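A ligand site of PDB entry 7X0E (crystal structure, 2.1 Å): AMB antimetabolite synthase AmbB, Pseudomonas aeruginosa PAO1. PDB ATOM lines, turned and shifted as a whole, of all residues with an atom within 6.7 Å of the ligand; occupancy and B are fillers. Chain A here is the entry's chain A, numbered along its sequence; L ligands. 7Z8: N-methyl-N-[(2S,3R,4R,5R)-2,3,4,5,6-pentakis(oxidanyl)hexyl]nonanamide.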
ATOM      1  N   VAL A 344     -34.061  -8.731  18.864  1.00  0.00           N
ATOM      2  CA  VAL A 344     -33.388  -9.095  17.625  1.00  0.00           C
ATOM      3  C   VAL A 344     -32.482 -10.298  17.847  1.00  0.00           C
ATOM      4  O   VAL A 344     -32.468 -11.246  17.060  1.00  0.00           O
ATOM      5  CB  VAL A 344     -32.619  -7.900  17.052  1.00  0.00           C
ATOM      6  CG1 VAL A 344     -31.729  -8.345  15.900  1.00  0.00           C
ATOM      7  CG2 VAL A 344     -33.578  -6.817  16.590  1.00  0.00           C
ATOM      8  N   LEU A 345     -31.695 -10.270  18.931  1.00  0.00           N
ATOM      9  CA  LEU A 345     -30.781 -11.373  19.201  1.00  0.00           C
ATOM     10  C   LEU A 345     -31.543 -12.639  19.571  1.00  0.00           C
ATOM     11  O   LEU A 345     -31.178 -13.735  19.133  1.00  0.00           O
ATOM     12  CB  LEU A 345     -29.814 -10.988  20.310  1.00  0.00           C
ATOM     13  CG  LEU A 345     -28.870  -9.833  19.984  1.00  0.00           C
ATOM     14  CD1 LEU A 345     -28.041  -9.473  21.191  1.00  0.00           C
ATOM     15  CD2 LEU A 345     -28.000 -10.186  18.790  1.00  0.00           C
ATOM     16  N   GLU A 348     -32.998 -14.282  16.458  1.00  0.00           N
ATOM     17  CA  GLU A 348     -31.977 -15.002  15.712  1.00  0.00           C
ATOM     18  C   GLU A 348     -31.503 -16.240  16.462  1.00  0.00           C
ATOM     19  O   GLU A 348     -31.156 -17.249  15.834  1.00  0.00           O
ATOM     20  CB  GLU A 348     -30.793 -14.078  15.423  1.00  0.00           C
ATOM     21  CG  GLU A 348     -31.066 -13.034  14.352  1.00  0.00           C
ATOM     22  CD  GLU A 348     -31.052 -13.613  12.953  1.00  0.00           C
ATOM     23  OE1 GLU A 348     -30.232 -14.516  12.695  1.00  0.00           O
ATOM     24  OE2 GLU A 348     -31.857 -13.163  12.105  1.00  0.00           O
ATOM     25  N   LEU A 349     -31.470 -16.182  17.793  1.00  0.00           N
ATOM     26  CA  LEU A 349     -30.997 -17.317  18.582  1.00  0.00           C
ATOM     27  C   LEU A 349     -32.043 -18.421  18.719  1.00  0.00           C
ATOM     28  O   LEU A 349     -31.681 -19.558  19.045  1.00  0.00           O
ATOM     29  CB  LEU A 349     -30.582 -16.836  19.980  1.00  0.00           C
ATOM     30  CG  LEU A 349     -29.193 -16.199  20.074  1.00  0.00           C
ATOM     31  CD1 LEU A 349     -29.037 -15.515  21.421  1.00  0.00           C
ATOM     32  CD2 LEU A 349     -28.107 -17.238  19.860  1.00  0.00           C
ATOM     33  N   ARG A 431     -23.322 -14.138  28.064  1.00  0.00           N
ATOM     34  CA  ARG A 431     -22.662 -14.060  26.763  1.00  0.00           C
ATOM     35  C   ARG A 431     -22.876 -12.726  26.068  1.00  0.00           C
ATOM     36  O   ARG A 431     -22.071 -12.375  25.196  1.00  0.00           O
ATOM     37  CB  ARG A 431     -23.174 -15.183  25.850  1.00  0.00           C
ATOM     38  CG  ARG A 431     -22.489 -16.524  26.055  1.00  0.00           C
ATOM     39  CD  ARG A 431     -23.128 -17.563  25.156  1.00  0.00           C
ATOM     40  NE  ARG A 431     -23.127 -17.144  23.765  1.00  0.00           N
ATOM     41  CZ  ARG A 431     -24.071 -17.459  22.883  1.00  0.00           C
ATOM     42  NH1 ARG A 431     -25.113 -18.185  23.232  1.00  0.00           N
ATOM     43  NH2 ARG A 431     -23.958 -17.025  21.638  1.00  0.00           N
ATOM     44  N   ILE A 432     -23.932 -11.994  26.420  1.00  0.00           N
ATOM     45  CA  ILE A 432     -24.287 -10.728  25.796  1.00  0.00           C
ATOM     46  C   ILE A 432     -24.430  -9.685  26.894  1.00  0.00           C
ATOM     47  O   ILE A 432     -24.852  -9.998  28.015  1.00  0.00           O
ATOM     48  CB  ILE A 432     -25.604 -10.856  25.006  1.00  0.00           C
ATOM     49  CG1 ILE A 432     -25.553 -12.080  24.087  1.00  0.00           C
ATOM     50  CG2 ILE A 432     -25.867  -9.609  24.193  1.00  0.00           C
ATOM     51  CD1 ILE A 432     -26.815 -12.293  23.276  1.00  0.00           C
ATOM     52  N   LEU A 463     -16.903 -11.053  25.868  1.00  0.00           N
ATOM     53  CA  LEU A 463     -18.259 -11.500  25.616  1.00  0.00           C
ATOM     54  C   LEU A 463     -18.505 -11.635  24.112  1.00  0.00           C
ATOM     55  O   LEU A 463     -17.771 -11.082  23.288  1.00  0.00           O
ATOM     56  CB  LEU A 463     -19.269 -10.516  26.225  1.00  0.00           C
ATOM     57  CG  LEU A 463     -19.132 -10.336  27.730  1.00  0.00           C
ATOM     58  CD1 LEU A 463     -20.123  -9.302  28.230  1.00  0.00           C
ATOM     59  CD2 LEU A 463     -19.333 -11.659  28.444  1.00  0.00           C
ATOM     60  N   ASP A 464     -19.542 -12.396  23.771  1.00  0.00           N
ATOM     61  CA  ASP A 464     -19.821 -12.654  22.365  1.00  0.00           C
ATOM     62  C   ASP A 464     -20.310 -11.399  21.649  1.00  0.00           C
ATOM     63  O   ASP A 464     -19.997 -11.184  20.473  1.00  0.00           O
ATOM     64  CB  ASP A 464     -20.848 -13.779  22.240  1.00  0.00           C
ATOM     65  CG  ASP A 464     -20.243 -15.141  22.530  1.00  0.00           C
ATOM     66  OD1 ASP A 464     -19.019 -15.231  22.734  1.00  0.00           O
ATOM     67  OD2 ASP A 464     -21.007 -16.130  22.545  1.00  0.00           O
ATOM     68  N   LEU A 465     -21.068 -10.542  22.351  1.00  0.00           N
ATOM     69  CA  LEU A 465     -21.600  -9.344  21.720  1.00  0.00           C
ATOM     70  C   LEU A 465     -21.995  -8.338  22.793  1.00  0.00           C
ATOM     71  O   LEU A 465     -22.661  -8.698  23.764  1.00  0.00           O
ATOM     72  CB  LEU A 465     -22.810  -9.666  20.841  1.00  0.00           C
ATOM     73  CG  LEU A 465     -23.433  -8.454  20.149  1.00  0.00           C
ATOM     74  CD1 LEU A 465     -22.527  -7.923  19.049  1.00  0.00           C
ATOM     75  CD2 LEU A 465     -24.800  -8.810  19.598  1.00  0.00           C
ATOM     76  N   VAL A 483     -17.548 -10.900  18.873  1.00  0.00           N
ATOM     77  CA  VAL A 483     -16.432 -11.824  18.715  1.00  0.00           C
ATOM     78  C   VAL A 483     -16.293 -12.184  17.246  1.00  0.00           C
ATOM     79  O   VAL A 483     -17.283 -12.423  16.535  1.00  0.00           O
ATOM     80  CB  VAL A 483     -16.634 -13.062  19.614  1.00  0.00           C
ATOM     81  CG1 VAL A 483     -17.885 -13.835  19.224  1.00  0.00           C
ATOM     82  CG2 VAL A 483     -15.403 -13.962  19.573  1.00  0.00           C
ATOM     83  N   ILE A 486     -17.980 -15.022  15.152  1.00  0.00           N
ATOM     84  CA  ILE A 486     -19.378 -14.933  14.763  1.00  0.00           C
ATOM     85  C   ILE A 486     -19.591 -13.723  13.866  1.00  0.00           C
ATOM     86  O   ILE A 486     -20.403 -13.774  12.927  1.00  0.00           O
ATOM     87  CB  ILE A 486     -20.290 -14.865  16.010  1.00  0.00           C
ATOM     88  CG1 ILE A 486     -20.172 -16.139  16.844  1.00  0.00           C
ATOM     89  CG2 ILE A 486     -21.743 -14.630  15.617  1.00  0.00           C
ATOM     90  CD1 ILE A 486     -20.628 -15.977  18.277  1.00  0.00           C
ATOM     91  N   PHE A 487     -18.864 -12.640  14.114  1.00  0.00           N
ATOM     92  CA  PHE A 487     -19.099 -11.366  13.451  1.00  0.00           C
ATOM     93  C   PHE A 487     -17.878 -10.928  12.657  1.00  0.00           C
ATOM     94  O   PHE A 487     -16.751 -11.000  13.167  1.00  0.00           O
ATOM     95  CB  PHE A 487     -19.452 -10.276  14.462  1.00  0.00           C
ATOM     96  CG  PHE A 487     -20.737 -10.507  15.196  1.00  0.00           C
ATOM     97  CD1 PHE A 487     -21.941 -10.084  14.664  1.00  0.00           C
ATOM     98  CD2 PHE A 487     -20.744 -11.152  16.418  1.00  0.00           C
ATOM     99  CE1 PHE A 487     -23.125 -10.300  15.340  1.00  0.00           C
ATOM    100  CE2 PHE A 487     -21.926 -11.376  17.109  1.00  0.00           C
ATOM    101  CZ  PHE A 487     -23.119 -10.947  16.558  1.00  0.00           C
ATOM    102  N   ARG A 491     -21.476  -8.087   9.064  1.00  0.00           N
ATOM    103  CA  ARG A 491     -22.580  -8.627   9.854  1.00  0.00           C
ATOM    104  C   ARG A 491     -22.997  -7.670  10.967  1.00  0.00           C
ATOM    105  O   ARG A 491     -24.173  -7.620  11.336  1.00  0.00           O
ATOM    106  CB  ARG A 491     -22.197  -9.988  10.448  1.00  0.00           C
ATOM    107  CG  ARG A 491     -23.388 -10.745  11.016  1.00  0.00           C
ATOM    108  CD  ARG A 491     -23.021 -12.164  11.446  1.00  0.00           C
ATOM    109  NE  ARG A 491     -24.214 -12.962  11.699  1.00  0.00           N
ATOM    110  CZ  ARG A 491     -24.190 -14.222  12.116  1.00  0.00           C
ATOM    111  NH1 ARG A 491     -23.055 -14.861  12.327  1.00  0.00           N
ATOM    112  NH2 ARG A 491     -25.345 -14.863  12.312  1.00  0.00           N
ATOM    113  N   ILE A 492     -22.039  -6.915  11.513  1.00  0.00           N
ATOM    114  CA  ILE A 492     -22.370  -5.931  12.536  1.00  0.00           C
ATOM    115  C   ILE A 492     -23.242  -4.824  11.961  1.00  0.00           C
ATOM    116  O   ILE A 492     -24.203  -4.372  12.598  1.00  0.00           O
ATOM    117  CB  ILE A 492     -21.087  -5.376  13.176  1.00  0.00           C
ATOM    118  CG1 ILE A 492     -20.417  -6.458  14.026  1.00  0.00           C
ATOM    119  CG2 ILE A 492     -21.388  -4.156  14.021  1.00  0.00           C
ATOM    120  CD1 ILE A 492     -19.136  -6.014  14.678  1.00  0.00           C
ATOM    121  N   GLU A 493     -22.931  -4.356  10.739  1.00  0.00           N
ATOM    122  CA  GLU A 493     -23.772  -3.358  10.105  1.00  0.00           C
ATOM    123  C   GLU A 493     -25.185  -3.880   9.881  1.00  0.00           C
ATOM    124  O   GLU A 493     -26.165  -3.148  10.100  1.00  0.00           O
ATOM    125  CB  GLU A 493     -23.142  -2.919   8.782  1.00  0.00           C
ATOM    126  CG  GLU A 493     -22.779  -1.446   8.713  1.00  0.00           C
ATOM    127  CD  GLU A 493     -23.832  -0.626   7.993  1.00  0.00           C
ATOM    128  OE1 GLU A 493     -24.899  -1.183   7.661  1.00  0.00           O
ATOM    129  OE2 GLU A 493     -23.587   0.578   7.747  1.00  0.00           O
ATOM    130  N   ARG A 494     -25.310  -5.144   9.462  1.00  0.00           N
ATOM    131  CA  ARG A 494     -26.626  -5.729   9.261  1.00  0.00           C
ATOM    132  C   ARG A 494     -27.362  -5.882  10.599  1.00  0.00           C
ATOM    133  O   ARG A 494     -28.582  -5.717  10.662  1.00  0.00           O
ATOM    134  CB  ARG A 494     -26.497  -7.068   8.555  1.00  0.00           C
ATOM    135  CG  ARG A 494     -25.914  -6.961   7.146  1.00  0.00           C
ATOM    136  CD  ARG A 494     -26.071  -8.247   6.345  1.00  0.00           C
ATOM    137  NE  ARG A 494     -25.483  -9.413   7.009  1.00  0.00           N
ATOM    138  CZ  ARG A 494     -24.223  -9.792   6.881  1.00  0.00           C
ATOM    139  NH1 ARG A 494     -23.362  -9.110   6.151  1.00  0.00           N
ATOM    140  NH2 ARG A 494     -23.815 -10.894   7.520  1.00  0.00           N
ATOM    141  N   LEU A 495     -26.617  -6.211  11.663  1.00  0.00           N
ATOM    142  CA  LEU A 495     -27.223  -6.309  12.985  1.00  0.00           C
ATOM    143  C   LEU A 495     -27.719  -4.943  13.467  1.00  0.00           C
ATOM    144  O   LEU A 495     -28.796  -4.853  14.068  1.00  0.00           O
ATOM    145  CB  LEU A 495     -26.216  -6.892  13.970  1.00  0.00           C
ATOM    146  CG  LEU A 495     -26.588  -6.874  15.453  1.00  0.00           C
ATOM    147  CD1 LEU A 495     -27.849  -7.687  15.692  1.00  0.00           C
ATOM    148  CD2 LEU A 495     -25.442  -7.400  16.291  1.00  0.00           C
ATOM    149  N   HIS A 496     -26.956  -3.886  13.206  1.00  0.00           N
ATOM    150  CA  HIS A 496     -27.380  -2.542  13.588  1.00  0.00           C
ATOM    151  C   HIS A 496     -28.657  -2.148  12.855  1.00  0.00           C
ATOM    152  O   HIS A 496     -29.545  -1.525  13.439  1.00  0.00           O
ATOM    153  CB  HIS A 496     -26.260  -1.551  13.308  1.00  0.00           C
ATOM    154  CG  HIS A 496     -26.632  -0.120  13.588  1.00  0.00           C
ATOM    155  ND1 HIS A 496     -26.434   0.467  14.821  1.00  0.00           N
ATOM    156  CD2 HIS A 496     -27.180   0.835  12.799  1.00  0.00           C
ATOM    157  CE1 HIS A 496     -26.852   1.724  14.777  1.00  0.00           C
ATOM    158  NE2 HIS A 496     -27.308   1.970  13.555  1.00  0.00           N
ATOM    159  N   GLN A 497     -28.755  -2.494  11.576  1.00  0.00           N
ATOM    160  CA  GLN A 497     -29.948  -2.143  10.804  1.00  0.00           C
ATOM    161  C   GLN A 497     -31.171  -2.907  11.296  1.00  0.00           C
ATOM    162  O   GLN A 497     -32.271  -2.354  11.383  1.00  0.00           O
ATOM    163  CB  GLN A 497     -29.714  -2.399   9.313  1.00  0.00           C
ATOM    164  CG  GLN A 497     -28.713  -1.453   8.683  1.00  0.00           C
ATOM    165  CD  GLN A 497     -28.554  -1.688   7.201  1.00  0.00           C
ATOM    166  OE1 GLN A 497     -27.501  -2.150   6.739  1.00  0.00           O
ATOM    167  NE2 GLN A 497     -29.591  -1.385   6.434  1.00  0.00           N
ATOM    168  N   ALA A 498     -31.001  -4.198  11.612  1.00  0.00           N
ATOM    169  CA  ALA A 498     -32.106  -4.968  12.175  1.00  0.00           C
ATOM    170  C   ALA A 498     -32.538  -4.401  13.524  1.00  0.00           C
ATOM    171  O   ALA A 498     -33.733  -4.419  13.859  1.00  0.00           O
ATOM    172  CB  ALA A 498     -31.698  -6.442  12.323  1.00  0.00           C
ATOM    173  N   TRP A 499     -31.584  -3.893  14.300  1.00  0.00           N
ATOM    174  CA  TRP A 499     -31.908  -3.281  15.588  1.00  0.00           C
ATOM    175  C   TRP A 499     -32.696  -1.987  15.409  1.00  0.00           C
ATOM    176  O   TRP A 499     -33.666  -1.731  16.129  1.00  0.00           O
ATOM    177  CB  TRP A 499     -30.630  -3.045  16.383  1.00  0.00           C
ATOM    178  CG  TRP A 499     -30.801  -2.274  17.650  1.00  0.00           C
ATOM    179  CD1 TRP A 499     -31.284  -2.734  18.843  1.00  0.00           C
ATOM    180  CD2 TRP A 499     -30.468  -0.897  17.873  1.00  0.00           C
ATOM    181  NE1 TRP A 499     -31.285  -1.731  19.787  1.00  0.00           N
ATOM    182  CE2 TRP A 499     -30.779  -0.591  19.213  1.00  0.00           C
ATOM    183  CE3 TRP A 499     -29.924   0.103  17.055  1.00  0.00           C
ATOM    184  CZ2 TRP A 499     -30.574   0.671  19.752  1.00  0.00           C
ATOM    185  CZ3 TRP A 499     -29.727   1.361  17.598  1.00  0.00           C
ATOM    186  CH2 TRP A 499     -30.054   1.629  18.937  1.00  0.00           C
ATOM    187  N   ARG A 501     -34.576  -1.254  12.782  1.00  0.00           N
ATOM    188  CA  ARG A 501     -35.896  -1.610  12.259  1.00  0.00           C
ATOM    189  C   ARG A 501     -36.817  -2.114  13.365  1.00  0.00           C
ATOM    190  O   ARG A 501     -37.996  -1.761  13.404  1.00  0.00           O
ATOM    191  CB  ARG A 501     -35.755  -2.666  11.167  1.00  0.00           C
ATOM    192  CG  ARG A 501     -35.248  -2.133   9.831  1.00  0.00           C
ATOM    193  CD  ARG A 501     -35.595  -3.087   8.715  1.00  0.00           C
ATOM    194  NE  ARG A 501     -35.140  -4.447   9.006  1.00  0.00           N
ATOM    195  CZ  ARG A 501     -33.943  -4.920   8.710  1.00  0.00           C
ATOM    196  NH1 ARG A 501     -33.033  -4.175   8.095  1.00  0.00           N
ATOM    197  NH2 ARG A 501     -33.643  -6.177   9.030  1.00  0.00           N
HETATM  198  C13 7Z8 L   1     -26.467 -13.840   8.513  1.00  0.00           C
HETATM  199  C12 7Z8 L   1     -25.236 -14.460  18.931  1.00  0.00           C
HETATM  200  C11 7Z8 L   1     -27.607 -10.665  12.800  1.00  0.00           C
HETATM  201  C10 7Z8 L   1     -26.287 -14.266  17.870  1.00  0.00           C
HETATM  202  C9  7Z8 L   1     -27.924 -11.404  14.078  1.00  0.00           C
HETATM  203  O1  7Z8 L   1     -29.934 -11.607   8.566  1.00  0.00           O
HETATM  204  O2  7Z8 L   1     -30.550  -9.371  10.012  1.00  0.00           O
HETATM  205  C3  7Z8 L   1     -27.655 -11.748   9.276  1.00  0.00           C
HETATM  206  C2  7Z8 L   1     -29.170  -9.721   9.826  1.00  0.00           C
HETATM  207  C6  7Z8 L   1     -27.079 -12.878  15.930  1.00  0.00           C
HETATM  208  C7  7Z8 L   1     -26.725 -12.001  14.741  1.00  0.00           C
HETATM  209  C8  7Z8 L   1     -25.916 -13.290  16.784  1.00  0.00           C
HETATM  210  C4  7Z8 L   1     -28.351  -9.174  10.994  1.00  0.00           C
HETATM  211  C1  7Z8 L   1     -29.046 -11.225   9.614  1.00  0.00           C
HETATM  212  N1  7Z8 L   1     -28.571  -9.895  12.250  1.00  0.00           N
HETATM  213  C5  7Z8 L   1     -27.546 -13.266   9.421  1.00  0.00           C
HETATM  214  C14 7Z8 L   1     -29.863  -9.732  12.905  1.00  0.00           C
HETATM  215  C15 7Z8 L   1     -24.983 -13.215  19.734  1.00  0.00           C
HETATM  216  C16 7Z8 L   1     -24.029 -13.444  20.882  1.00  0.00           C
HETATM  217  O3  7Z8 L   1     -27.381 -11.398   7.922  1.00  0.00           O
HETATM  218  O4  7Z8 L   1     -27.269 -13.599  10.783  1.00  0.00           O
HETATM  219  O5  7Z8 L   1     -26.492 -10.779  12.275  1.00  0.00           O
HETATM  220  O6  7Z8 L   1     -25.216 -13.186   8.745  1.00  0.00           O
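Merely in contact with the ligand: Asp 464, Leu 495, Glu 348, Phe 487, Arg 431, Val 344, Ile 432, Ala 498 and Leu 465. Hydrophobic or aromatic side chains within 4 Å of the ligand: Val 344, Ile 432, Leu 465, Phe 487 and Ala 498. Within 4 Å of the ligand: Val 344, Glu 348, Arg 431, Ile 432, Asp 464, Leu 465, Phe 487, Arg 491, Arg 494, Leu 495 and Ala 498.
The backbone carbonyl oxygen of Asp 464 lies within hydrogen-bond range of the backbone NH of Val 483. OD2 of Asp 464 lies within salt-bridge range of NE of Arg 431 (2.6 Å). The backbone carbonyl oxygen of Ile 486 sits at hydrogen-bond distance from the guanidinium group of Arg 491 (2.9 Å).
An oxygen (O4) of the ligand is in hydrogen-bond range of the guanidinium group of Arg 491, at 2.8 Å. O3 of the ligand is in hydrogen-bond range of NE of Arg 494 (2.9 Å).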
